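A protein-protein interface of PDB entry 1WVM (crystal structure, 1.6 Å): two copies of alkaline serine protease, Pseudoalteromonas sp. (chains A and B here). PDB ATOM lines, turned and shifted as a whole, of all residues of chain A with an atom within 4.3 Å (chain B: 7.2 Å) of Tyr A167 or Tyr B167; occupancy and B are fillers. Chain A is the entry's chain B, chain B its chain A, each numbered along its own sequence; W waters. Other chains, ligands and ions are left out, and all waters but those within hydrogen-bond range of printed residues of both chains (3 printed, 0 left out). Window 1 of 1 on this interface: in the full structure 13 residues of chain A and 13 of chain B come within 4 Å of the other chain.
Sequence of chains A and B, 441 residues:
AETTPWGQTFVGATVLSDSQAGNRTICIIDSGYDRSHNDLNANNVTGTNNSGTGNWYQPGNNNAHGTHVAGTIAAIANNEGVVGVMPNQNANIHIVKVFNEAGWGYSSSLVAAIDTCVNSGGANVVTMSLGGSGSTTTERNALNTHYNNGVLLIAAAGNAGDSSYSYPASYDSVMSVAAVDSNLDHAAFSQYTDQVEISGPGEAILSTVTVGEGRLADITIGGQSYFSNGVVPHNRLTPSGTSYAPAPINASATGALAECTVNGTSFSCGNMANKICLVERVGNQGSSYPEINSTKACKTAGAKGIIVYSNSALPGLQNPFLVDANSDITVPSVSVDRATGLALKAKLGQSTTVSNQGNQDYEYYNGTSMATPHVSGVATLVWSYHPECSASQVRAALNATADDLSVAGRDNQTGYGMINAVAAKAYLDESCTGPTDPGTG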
ATOM      1  N   LEU A 130      19.272  -2.955  -6.112  1.00  0.00           N
ATOM      2  CA  LEU A 130      19.371  -4.288  -6.674  1.00  0.00           C
ATOM      3  C   LEU A 130      19.587  -4.174  -8.170  1.00  0.00           C
ATOM      4  O   LEU A 130      19.521  -3.082  -8.739  1.00  0.00           O
ATOM      5  CB  LEU A 130      18.066  -5.051  -6.398  1.00  0.00           C
ATOM      6  CG  LEU A 130      16.766  -4.301  -6.730  1.00  0.00           C
ATOM      7  CD1 LEU A 130      16.538  -4.277  -8.234  1.00  0.00           C
ATOM      8  CD2 LEU A 130      15.596  -4.981  -6.033  1.00  0.00           C
ATOM      9  N   GLY A 131      19.843  -5.307  -8.808  1.00  0.00           N
ATOM     10  CA  GLY A 131      20.039  -5.287 -10.241  1.00  0.00           C
ATOM     11  C   GLY A 131      20.504  -6.612 -10.794  1.00  0.00           C
ATOM     12  O   GLY A 131      20.652  -7.597 -10.068  1.00  0.00           O
ATOM     13  N   GLY A 132      20.729  -6.625 -12.100  1.00  0.00           N
ATOM     14  CA  GLY A 132      21.186  -7.822 -12.775  1.00  0.00           C
ATOM     15  C   GLY A 132      22.029  -7.407 -13.960  1.00  0.00           C
ATOM     16  O   GLY A 132      22.095  -6.230 -14.297  1.00  0.00           O
ATOM     17  N   SER A 133      22.669  -8.373 -14.604  1.00  0.00           N
ATOM     18  CA  SER A 133      23.514  -8.069 -15.749  1.00  0.00           C
ATOM     19  C   SER A 133      22.730  -7.953 -17.051  1.00  0.00           C
ATOM     20  O   SER A 133      23.197  -7.335 -18.005  1.00  0.00           O
ATOM     21  CB  SER A 133      24.590  -9.147 -15.889  1.00  0.00           C
ATOM     22  OG  SER A 133      24.001 -10.434 -15.900  1.00  0.00           O
ATOM     23  N   GLY A 134      21.536  -8.538 -17.081  1.00  0.00           N
ATOM     24  CA  GLY A 134      20.723  -8.501 -18.284  1.00  0.00           C
ATOM     25  C   GLY A 134      19.923  -7.232 -18.510  1.00  0.00           C
ATOM     26  O   GLY A 134      19.578  -6.516 -17.569  1.00  0.00           O
ATOM     27  N   SER A 135      19.629  -6.957 -19.775  1.00  0.00           N
ATOM     28  CA  SER A 135      18.848  -5.784 -20.157  1.00  0.00           C
ATOM     29  C   SER A 135      17.866  -6.187 -21.254  1.00  0.00           C
ATOM     30  O   SER A 135      18.158  -7.074 -22.056  1.00  0.00           O
ATOM     31  CB  SER A 135      19.777  -4.661 -20.646  1.00  0.00           C
ATOM     32  OG  SER A 135      20.734  -5.131 -21.587  1.00  0.00           O
ATOM     33  N   TYR A 165      27.804  -3.102 -16.766  1.00  0.00           N
ATOM     34  CA  TYR A 165      26.544  -2.395 -16.582  1.00  0.00           C
ATOM     35  C   TYR A 165      25.574  -3.257 -15.796  1.00  0.00           C
ATOM     36  O   TYR A 165      25.329  -4.408 -16.155  1.00  0.00           O
ATOM     37  CB  TYR A 165      25.893  -2.088 -17.934  1.00  0.00           C
ATOM     38  CG  TYR A 165      26.614  -1.073 -18.784  1.00  0.00           C
ATOM     39  CD1 TYR A 165      26.727   0.256 -18.380  1.00  0.00           C
ATOM     40  CD2 TYR A 165      27.156  -1.436 -20.020  1.00  0.00           C
ATOM     41  CE1 TYR A 165      27.358   1.202 -19.187  1.00  0.00           C
ATOM     42  CE2 TYR A 165      27.787  -0.500 -20.829  1.00  0.00           C
ATOM     43  CZ  TYR A 165      27.883   0.814 -20.410  1.00  0.00           C
ATOM     44  OH  TYR A 165      28.492   1.737 -21.222  1.00  0.00           O
ATOM     45  N   SER A 166      25.032  -2.712 -14.714  1.00  0.00           N
ATOM     46  CA  SER A 166      24.028  -3.434 -13.948  1.00  0.00           C
ATOM     47  C   SER A 166      22.740  -2.688 -14.259  1.00  0.00           C
ATOM     48  O   SER A 166      22.745  -1.465 -14.407  1.00  0.00           O
ATOM     49  CB  SER A 166      24.327  -3.391 -12.448  1.00  0.00           C
ATOM     50  OG  SER A 166      25.422  -4.238 -12.137  1.00  0.00           O
ATOM     51  N   TYR A 167      21.653  -3.434 -14.397  1.00  0.00           N
ATOM     52  CA  TYR A 167      20.350  -2.865 -14.705  1.00  0.00           C
ATOM     53  C   TYR A 167      19.438  -3.145 -13.520  1.00  0.00           C
ATOM     54  O   TYR A 167      19.573  -4.177 -12.860  1.00  0.00           O
ATOM     55  CB  TYR A 167      19.821  -3.509 -15.988  1.00  0.00           C
ATOM     56  CG  TYR A 167      20.707  -3.214 -17.178  1.00  0.00           C
ATOM     57  CD1 TYR A 167      20.528  -2.056 -17.933  1.00  0.00           C
ATOM     58  CD2 TYR A 167      21.773  -4.055 -17.502  1.00  0.00           C
ATOM     59  CE1 TYR A 167      21.390  -1.736 -18.982  1.00  0.00           C
ATOM     60  CE2 TYR A 167      22.643  -3.744 -18.547  1.00  0.00           C
ATOM     61  CZ  TYR A 167      22.446  -2.585 -19.280  1.00  0.00           C
ATOM     62  OH  TYR A 167      23.304  -2.265 -20.307  1.00  0.00           O
ATOM     63  N   PRO A 168      18.441  -2.280 -13.277  1.00  0.00           N
ATOM     64  CA  PRO A 168      18.033  -1.058 -13.983  1.00  0.00           C
ATOM     65  C   PRO A 168      18.910   0.193 -13.944  1.00  0.00           C
ATOM     66  O   PRO A 168      18.669   1.135 -14.702  1.00  0.00           O
ATOM     67  CB  PRO A 168      16.652  -0.788 -13.396  1.00  0.00           C
ATOM     68  CG  PRO A 168      16.852  -1.180 -11.951  1.00  0.00           C
ATOM     69  CD  PRO A 168      17.610  -2.493 -12.074  1.00  0.00           C
ATOM     70  N   ALA A 169      19.915   0.221 -13.079  1.00  0.00           N
ATOM     71  CA  ALA A 169      20.758   1.405 -12.977  1.00  0.00           C
ATOM     72  C   ALA A 169      21.272   1.935 -14.310  1.00  0.00           C
ATOM     73  O   ALA A 169      21.298   3.147 -14.541  1.00  0.00           O
ATOM     74  CB  ALA A 169      21.936   1.122 -12.057  1.00  0.00           C
ATOM     75  N   SER A 170      21.667   1.030 -15.196  1.00  0.00           N
ATOM     76  CA  SER A 170      22.241   1.446 -16.467  1.00  0.00           C
ATOM     77  C   SER A 170      21.309   1.853 -17.609  1.00  0.00           C
ATOM     78  O   SER A 170      21.762   2.054 -18.737  1.00  0.00           O
ATOM     79  CB  SER A 170      23.242   0.383 -16.928  1.00  0.00           C
ATOM     80  OG  SER A 170      24.269   0.245 -15.949  1.00  0.00           O
ATOM     81  N   TYR A 171      20.012   1.969 -17.328  1.00  0.00           N
ATOM     82  CA  TYR A 171      19.068   2.443 -18.340  1.00  0.00           C
ATOM     83  C   TYR A 171      19.102   3.973 -18.247  1.00  0.00           C
ATOM     84  O   TYR A 171      19.339   4.524 -17.173  1.00  0.00           O
ATOM     85  CB  TYR A 171      17.646   1.959 -18.050  1.00  0.00           C
ATOM     86  CG  TYR A 171      17.414   0.487 -18.288  1.00  0.00           C
ATOM     87  CD1 TYR A 171      16.897  -0.326 -17.277  1.00  0.00           C
ATOM     88  CD2 TYR A 171      17.672  -0.091 -19.532  1.00  0.00           C
ATOM     89  CE1 TYR A 171      16.642  -1.672 -17.498  1.00  0.00           C
ATOM     90  CE2 TYR A 171      17.417  -1.439 -19.767  1.00  0.00           C
ATOM     91  CZ  TYR A 171      16.902  -2.222 -18.746  1.00  0.00           C
ATOM     92  OH  TYR A 171      16.638  -3.550 -18.964  1.00  0.00           O
ATOM     93  N   LEU B 110      36.333 -11.137 -26.154  1.00  0.00           N
ATOM     94  CA  LEU B 110      35.767 -10.883 -27.471  1.00  0.00           C
ATOM     95  C   LEU B 110      36.515  -9.680 -28.041  1.00  0.00           C
ATOM     96  O   LEU B 110      36.821  -9.630 -29.229  1.00  0.00           O
ATOM     97  CB  LEU B 110      34.271 -10.564 -27.359  1.00  0.00           C
ATOM     98  CG  LEU B 110      33.581 -10.144 -28.662  1.00  0.00           C
ATOM     99  CD1 LEU B 110      33.649 -11.282 -29.666  1.00  0.00           C
ATOM    100  CD2 LEU B 110      32.135  -9.765 -28.384  1.00  0.00           C
ATOM    101  N   LEU B 130      27.189 -14.598 -32.591  1.00  0.00           N
ATOM    102  CA  LEU B 130      27.283 -15.030 -31.208  1.00  0.00           C
ATOM    103  C   LEU B 130      26.960 -13.861 -30.299  1.00  0.00           C
ATOM    104  O   LEU B 130      26.784 -12.732 -30.763  1.00  0.00           O
ATOM    105  CB  LEU B 130      28.708 -15.526 -30.928  1.00  0.00           C
ATOM    106  CG  LEU B 130      29.851 -14.640 -31.447  1.00  0.00           C
ATOM    107  CD1 LEU B 130      29.991 -13.395 -30.589  1.00  0.00           C
ATOM    108  CD2 LEU B 130      31.155 -15.428 -31.438  1.00  0.00           C
ATOM    109  N   GLY B 131      26.882 -14.130 -29.003  1.00  0.00           N
ATOM    110  CA  GLY B 131      26.591 -13.062 -28.073  1.00  0.00           C
ATOM    111  C   GLY B 131      26.368 -13.526 -26.655  1.00  0.00           C
ATOM    112  O   GLY B 131      26.398 -14.721 -26.356  1.00  0.00           O
ATOM    113  N   GLY B 132      26.146 -12.554 -25.780  1.00  0.00           N
ATOM    114  CA  GLY B 132      25.908 -12.833 -24.379  1.00  0.00           C
ATOM    115  C   GLY B 132      24.938 -11.795 -23.859  1.00  0.00           C
ATOM    116  O   GLY B 132      24.666 -10.808 -24.535  1.00  0.00           O
ATOM    117  N   SER B 133      24.423 -12.006 -22.656  1.00  0.00           N
ATOM    118  CA  SER B 133      23.461 -11.074 -22.087  1.00  0.00           C
ATOM    119  C   SER B 133      24.104  -9.878 -21.399  1.00  0.00           C
ATOM    120  O   SER B 133      23.464  -8.843 -21.222  1.00  0.00           O
ATOM    121  CB  SER B 133      22.568 -11.810 -21.091  1.00  0.00           C
ATOM    122  OG  SER B 133      23.354 -12.431 -20.089  1.00  0.00           O
ATOM    123  N   GLY B 134      25.368 -10.017 -21.016  1.00  0.00           N
ATOM    124  CA  GLY B 134      26.048  -8.934 -20.327  1.00  0.00           C
ATOM    125  C   GLY B 134      26.622  -7.841 -21.207  1.00  0.00           C
ATOM    126  O   GLY B 134      26.904  -8.057 -22.385  1.00  0.00           O
ATOM    127  N   SER B 135      26.791  -6.659 -20.622  1.00  0.00           N
ATOM    128  CA  SER B 135      27.351  -5.512 -21.328  1.00  0.00           C
ATOM    129  C   SER B 135      28.282  -4.749 -20.388  1.00  0.00           C
ATOM    130  O   SER B 135      28.039  -4.700 -19.182  1.00  0.00           O
ATOM    131  CB  SER B 135      26.228  -4.594 -21.835  1.00  0.00           C
ATOM    132  OG  SER B 135      25.275  -4.305 -20.818  1.00  0.00           O
ATOM    133  N   THR B 136      29.351  -4.169 -20.930  1.00  0.00           N
ATOM    134  CA  THR B 136      30.293  -3.408 -20.110  1.00  0.00           C
ATOM    135  C   THR B 136      30.744  -2.128 -20.808  1.00  0.00           C
ATOM    136  O   THR B 136      30.669  -2.014 -22.033  1.00  0.00           O
ATOM    137  CB  THR B 136      31.552  -4.239 -19.750  1.00  0.00           C
ATOM    138  OG1 THR B 136      32.440  -4.292 -20.876  1.00  0.00           O
ATOM    139  CG2 THR B 136      31.164  -5.650 -19.354  1.00  0.00           C
ATOM    140  N   GLU B 139      33.994  -2.693 -22.966  1.00  0.00           N
ATOM    141  CA  GLU B 139      33.714  -3.352 -24.238  1.00  0.00           C
ATOM    142  C   GLU B 139      33.020  -2.387 -25.196  1.00  0.00           C
ATOM    143  O   GLU B 139      33.362  -2.318 -26.377  1.00  0.00           O
ATOM    144  CB  GLU B 139      32.858  -4.597 -24.005  1.00  0.00           C
ATOM    145  CG  GLU B 139      32.553  -5.405 -25.260  1.00  0.00           C
ATOM    146  CD  GLU B 139      31.967  -6.761 -24.926  1.00  0.00           C
ATOM    147  OE1 GLU B 139      32.710  -7.764 -24.966  1.00  0.00           O
ATOM    148  OE2 GLU B 139      30.764  -6.822 -24.599  1.00  0.00           O
ATOM    149  N   LEU B 143      34.675  -1.369 -28.890  1.00  0.00           N
ATOM    150  CA  LEU B 143      34.007  -1.594 -30.165  1.00  0.00           C
ATOM    151  C   LEU B 143      33.685  -0.279 -30.862  1.00  0.00           C
ATOM    152  O   LEU B 143      33.757  -0.188 -32.087  1.00  0.00           O
ATOM    153  CB  LEU B 143      32.737  -2.426 -29.968  1.00  0.00           C
ATOM    154  CG  LEU B 143      32.979  -3.944 -29.968  1.00  0.00           C
ATOM    155  CD1 LEU B 143      34.015  -4.316 -28.915  1.00  0.00           C
ATOM    156  CD2 LEU B 143      31.667  -4.670 -29.717  1.00  0.00           C
ATOM    157  N   ALA B 155      26.541  -8.258 -35.902  1.00  0.00           N
ATOM    158  CA  ALA B 155      26.309  -9.390 -35.009  1.00  0.00           C
ATOM    159  C   ALA B 155      24.853  -9.833 -34.946  1.00  0.00           C
ATOM    160  O   ALA B 155      23.939  -9.067 -35.265  1.00  0.00           O
ATOM    161  CB  ALA B 155      26.813  -9.047 -33.602  1.00  0.00           C
ATOM    162  N   ALA B 156      24.650 -11.075 -34.514  1.00  0.00           N
ATOM    163  CA  ALA B 156      23.318 -11.671 -34.400  1.00  0.00           C
ATOM    164  C   ALA B 156      22.527 -11.141 -33.203  1.00  0.00           C
ATOM    165  O   ALA B 156      23.075 -10.955 -32.119  1.00  0.00           O
ATOM    166  CB  ALA B 156      23.448 -13.188 -34.300  1.00  0.00           C
ATOM    167  N   ALA B 157      21.229 -10.927 -33.405  1.00  0.00           N
ATOM    168  CA  ALA B 157      20.356 -10.418 -32.345  1.00  0.00           C
ATOM    169  C   ALA B 157      20.051 -11.443 -31.247  1.00  0.00           C
ATOM    170  O   ALA B 157      19.719 -11.069 -30.121  1.00  0.00           O
ATOM    171  CB  ALA B 157      19.050  -9.908 -32.949  1.00  0.00           C
ATOM    172  N   SER B 164      15.025  -9.333 -25.054  1.00  0.00           N
ATOM    173  CA  SER B 164      16.317  -9.128 -24.415  1.00  0.00           C
ATOM    174  C   SER B 164      17.400  -8.681 -25.383  1.00  0.00           C
ATOM    175  O   SER B 164      17.377  -9.011 -26.572  1.00  0.00           O
ATOM    176  CB  SER B 164      16.771 -10.396 -23.683  1.00  0.00           C
ATOM    177  OG  SER B 164      17.063 -11.448 -24.583  1.00  0.00           O
ATOM    178  N   TYR B 165      18.338  -7.904 -24.857  1.00  0.00           N
ATOM    179  CA  TYR B 165      19.459  -7.410 -25.639  1.00  0.00           C
ATOM    180  C   TYR B 165      20.595  -8.413 -25.556  1.00  0.00           C
ATOM    181  O   TYR B 165      20.978  -8.842 -24.468  1.00  0.00           O
ATOM    182  CB  TYR B 165      19.981  -6.085 -25.078  1.00  0.00           C
ATOM    183  CG  TYR B 165      19.052  -4.907 -25.226  1.00  0.00           C
ATOM    184  CD1 TYR B 165      18.794  -4.345 -26.475  1.00  0.00           C
ATOM    185  CD2 TYR B 165      18.454  -4.333 -24.106  1.00  0.00           C
ATOM    186  CE1 TYR B 165      17.963  -3.235 -26.608  1.00  0.00           C
ATOM    187  CE2 TYR B 165      17.625  -3.228 -24.226  1.00  0.00           C
ATOM    188  CZ  TYR B 165      17.384  -2.682 -25.475  1.00  0.00           C
ATOM    189  OH  TYR B 165      16.568  -1.577 -25.587  1.00  0.00           O
ATOM    190  N   SER B 166      21.119  -8.801 -26.710  1.00  0.00           N
ATOM    191  CA  SER B 166      22.262  -9.696 -26.750  1.00  0.00           C
ATOM    192  C   SER B 166      23.398  -8.804 -27.225  1.00  0.00           C
ATOM    193  O   SER B 166      23.200  -7.942 -28.080  1.00  0.00           O
ATOM    194  CB  SER B 166      22.031 -10.850 -27.730  1.00  0.00           C
ATOM    195  OG  SER B 166      21.167 -11.821 -27.161  1.00  0.00           O
ATOM    196  N   TYR B 167      24.573  -8.979 -26.635  1.00  0.00           N
ATOM    197  CA  TYR B 167      25.737  -8.181 -26.995  1.00  0.00           C
ATOM    198  C   TYR B 167      26.746  -9.123 -27.631  1.00  0.00           C
ATOM    199  O   TYR B 167      26.808 -10.302 -27.278  1.00  0.00           O
ATOM    200  CB  TYR B 167      26.292  -7.507 -25.736  1.00  0.00           C
ATOM    201  CG  TYR B 167      25.300  -6.539 -25.123  1.00  0.00           C
ATOM    202  CD1 TYR B 167      25.294  -5.190 -25.484  1.00  0.00           C
ATOM    203  CD2 TYR B 167      24.321  -6.988 -24.235  1.00  0.00           C
ATOM    204  CE1 TYR B 167      24.332  -4.308 -24.975  1.00  0.00           C
ATOM    205  CE2 TYR B 167      23.355  -6.119 -23.723  1.00  0.00           C
ATOM    206  CZ  TYR B 167      23.367  -4.785 -24.099  1.00  0.00           C
ATOM    207  OH  TYR B 167      22.404  -3.925 -23.604  1.00  0.00           O
ATOM    208  N   PRO B 168      27.602  -8.609 -28.526  1.00  0.00           N
ATOM    209  CA  PRO B 168      27.756  -7.232 -29.013  1.00  0.00           C
ATOM    210  C   PRO B 168      26.696  -6.600 -29.922  1.00  0.00           C
ATOM    211  O   PRO B 168      26.749  -5.393 -30.174  1.00  0.00           O
ATOM    212  CB  PRO B 168      29.117  -7.281 -29.696  1.00  0.00           C
ATOM    213  CG  PRO B 168      29.080  -8.629 -30.342  1.00  0.00           C
ATOM    214  CD  PRO B 168      28.521  -9.517 -29.241  1.00  0.00           C
ATOM    215  N   ALA B 169      25.742  -7.384 -30.409  1.00  0.00           N
ATOM    216  CA  ALA B 169      24.727  -6.846 -31.309  1.00  0.00           C
ATOM    217  C   ALA B 169      24.045  -5.578 -30.807  1.00  0.00           C
ATOM    218  O   ALA B 169      23.809  -4.652 -31.579  1.00  0.00           O
ATOM    219  CB  ALA B 169      23.671  -7.907 -31.602  1.00  0.00           C
ATOM    220  N   SER B 170      23.756  -5.526 -29.512  1.00  0.00           N
ATOM    221  CA  SER B 170      23.040  -4.386 -28.954  1.00  0.00           C
ATOM    222  C   SER B 170      23.820  -3.118 -28.612  1.00  0.00           C
ATOM    223  O   SER B 170      23.270  -2.198 -28.001  1.00  0.00           O
ATOM    224  CB  SER B 170      22.221  -4.852 -27.751  1.00  0.00           C
ATOM    225  OG  SER B 170      21.305  -5.861 -28.157  1.00  0.00           O
ATOM    226  N   TYR B 171      25.093  -3.062 -28.994  1.00  0.00           N
ATOM    227  CA  TYR B 171      25.892  -1.858 -28.775  1.00  0.00           C
ATOM    228  C   TYR B 171      25.611  -0.961 -29.986  1.00  0.00           C
ATOM    229  O   TYR B 171      25.334  -1.465 -31.078  1.00  0.00           O
ATOM    230  CB  TYR B 171      27.388  -2.191 -28.726  1.00  0.00           C
ATOM    231  CG  TYR B 171      27.852  -2.876 -27.460  1.00  0.00           C
ATOM    232  CD1 TYR B 171      28.549  -4.084 -27.516  1.00  0.00           C
ATOM    233  CD2 TYR B 171      27.639  -2.298 -26.209  1.00  0.00           C
ATOM    234  CE1 TYR B 171      29.027  -4.697 -26.361  1.00  0.00           C
ATOM    235  CE2 TYR B 171      28.115  -2.902 -25.048  1.00  0.00           C
ATOM    236  CZ  TYR B 171      28.808  -4.100 -25.130  1.00  0.00           C
ATOM    237  OH  TYR B 171      29.300  -4.693 -23.988  1.00  0.00           O
ATOM    238  N   ASP B 172      25.678   0.356 -29.808  1.00  0.00           N
ATOM    239  CA  ASP B 172      25.415   1.278 -30.916  1.00  0.00           C
ATOM    240  C   ASP B 172      26.398   1.142 -32.082  1.00  0.00           C
ATOM    241  O   ASP B 172      26.071   1.483 -33.221  1.00  0.00           O
ATOM    242  CB  ASP B 172      25.448   2.735 -30.438  1.00  0.00           C
ATOM    243  CG  ASP B 172      24.374   3.049 -29.413  1.00  0.00           C
ATOM    244  OD1 ASP B 172      23.302   2.412 -29.442  1.00  0.00           O
ATOM    245  OD2 ASP B 172      24.600   3.958 -28.586  1.00  0.00           O
ATOM    246  N   GLN B 191      15.146 -12.484 -31.509  1.00  0.00           N
ATOM    247  CA  GLN B 191      14.938 -11.471 -30.483  1.00  0.00           C
ATOM    248  C   GLN B 191      14.592 -10.126 -31.102  1.00  0.00           C
ATOM    249  O   GLN B 191      15.201  -9.701 -32.084  1.00  0.00           O
ATOM    250  CB  GLN B 191      16.174 -11.360 -29.588  1.00  0.00           C
ATOM    251  CG  GLN B 191      16.245 -12.485 -28.568  1.00  0.00           C
ATOM    252  CD  GLN B 191      17.598 -12.611 -27.903  1.00  0.00           C
ATOM    253  OE1 GLN B 191      18.125 -11.649 -27.335  1.00  0.00           O
ATOM    254  NE2 GLN B 191      18.166 -13.806 -27.958  1.00  0.00           N
ATOM    255  N   GLN B 195      17.282  -2.166 -30.975  1.00  0.00           N
ATOM    256  CA  GLN B 195      18.630  -2.162 -31.533  1.00  0.00           C
ATOM    257  C   GLN B 195      18.606  -2.908 -32.868  1.00  0.00           C
ATOM    258  O   GLN B 195      19.422  -2.622 -33.746  1.00  0.00           O
ATOM    259  CB  GLN B 195      19.624  -2.839 -30.584  1.00  0.00           C
ATOM    260  CG  GLN B 195      20.220  -1.922 -29.505  1.00  0.00           C
ATOM    261  CD  GLN B 195      21.249  -0.935 -30.048  1.00  0.00           C
ATOM    262  OE1 GLN B 195      22.081  -1.280 -30.893  1.00  0.00           O
ATOM    263  NE2 GLN B 195      21.214   0.295 -29.541  1.00  0.00           N
HETATM  264  O   HOH W   1      25.827  -6.490 -17.883  1.00  0.00           O
HETATM  265  O   HOH W   2      23.198  -6.238 -20.466  1.00  0.00           O
HETATM  266  O   HOH W   3      20.818  -8.727 -21.749  1.00  0.00           O
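N of Tyr B165 is in hydrogen-bond range of O of Ser A135 (2.9 Å).
The side-chain hydroxyl (OH) of Tyr A167 is in hydrogen-bond range of the side-chain hydroxyl (OG) of Ser B135 (2.9 Å).
N of Tyr A165 is in hydrogen-bond range of O of Ser B135, 2.9 Å away.
OH of Tyr B167 lies within hydrogen-bond range of OG of Ser A135 (2.9 Å).
The backbone NH of Gly A132 is in hydrogen-bond range of the backbone carbonyl oxygen of Tyr A167, at 2.8 Å.
OH of Tyr B171 sits at hydrogen-bond distance from N of Thr B136 (3.1 Å).
O of Ser B164 sits close to OE1 of Gln B191, at 2.8 Å.
N of Gly B132 is in hydrogen-bond range of O of Tyr B167, at 2.8 Å.
OG1 of Thr B136 lies within hydrogen-bond range of N of Glu B139 (3.1 Å).
Ser B133 touches Ser A133.
Ser A135 touches Ser B164.
CE2 of Tyr A165 touches C of Thr B136 (3.4 Å).
Tyr A167 touches Tyr B167 (OH to OH, 3.8 Å).
Tyr A167 touches two residues of chain B.
Tyr B167 touches just these residues of chain A: Ser A135 (2.9 Å) and Tyr A167 (3.8 Å).
Of the printed residues of chain A, Ser B135 touches Tyr A165 (2.9 Å) and Tyr A167 (2.9 Å).
Printed residues of chain A within 4 Å of Tyr B165: Ser A135.
Leu A130 touches none of the printed residues of chain B.
The nearest printed residue of chain A that does not touch Tyr B167 is Ser A133 (5.8 Å).
Of the 24 printed residues of chain B, 6 touch a printed residue of chain A.
Printed residues of chain B that touch a printed residue of chain A: Ser B133, Ser B135, Thr B136, Ser B164, Tyr B165 and Tyr B167.
Along chain B the printed residues that touch a printed residue of chain A span positions 133 to 167.
Among the printed residues, 8 pairs touch across the chains.
Ser B133 touches its own counterpart, Ser A133.
Ser A135 touches Tyr B165, and with the chains exchanged Tyr A165 touches Ser B135.
Ser A135 touches Tyr B167, and with the chains exchanged Tyr A167 touches Ser B135.
Tyr A167 touches its own counterpart, Tyr B167.
Of the 8 pairs that touch across the chains among the printed residues, 6 have their exchanged pair printed and touching as well.
Water W2 lies within hydrogen-bond range of O of Ser A133, O of Ser B133, OG of Ser B135 and OG of Ser A135.
Water W3 lies within hydrogen-bond range of the backbone carbonyl oxygen of Ser B133 (2.7 Å), the backbone carbonyl oxygen of Tyr B165 (2.7 Å) and the backbone NH of Ser A135 (2.9 Å).
Water W1 lies within hydrogen-bond range of the backbone carbonyl oxygen (O) of Tyr A165 (2.8 Å), the backbone carbonyl oxygen (O) of Ser A133 (2.8 Å) and the backbone NH (N) of Ser B135 (2.9 Å).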
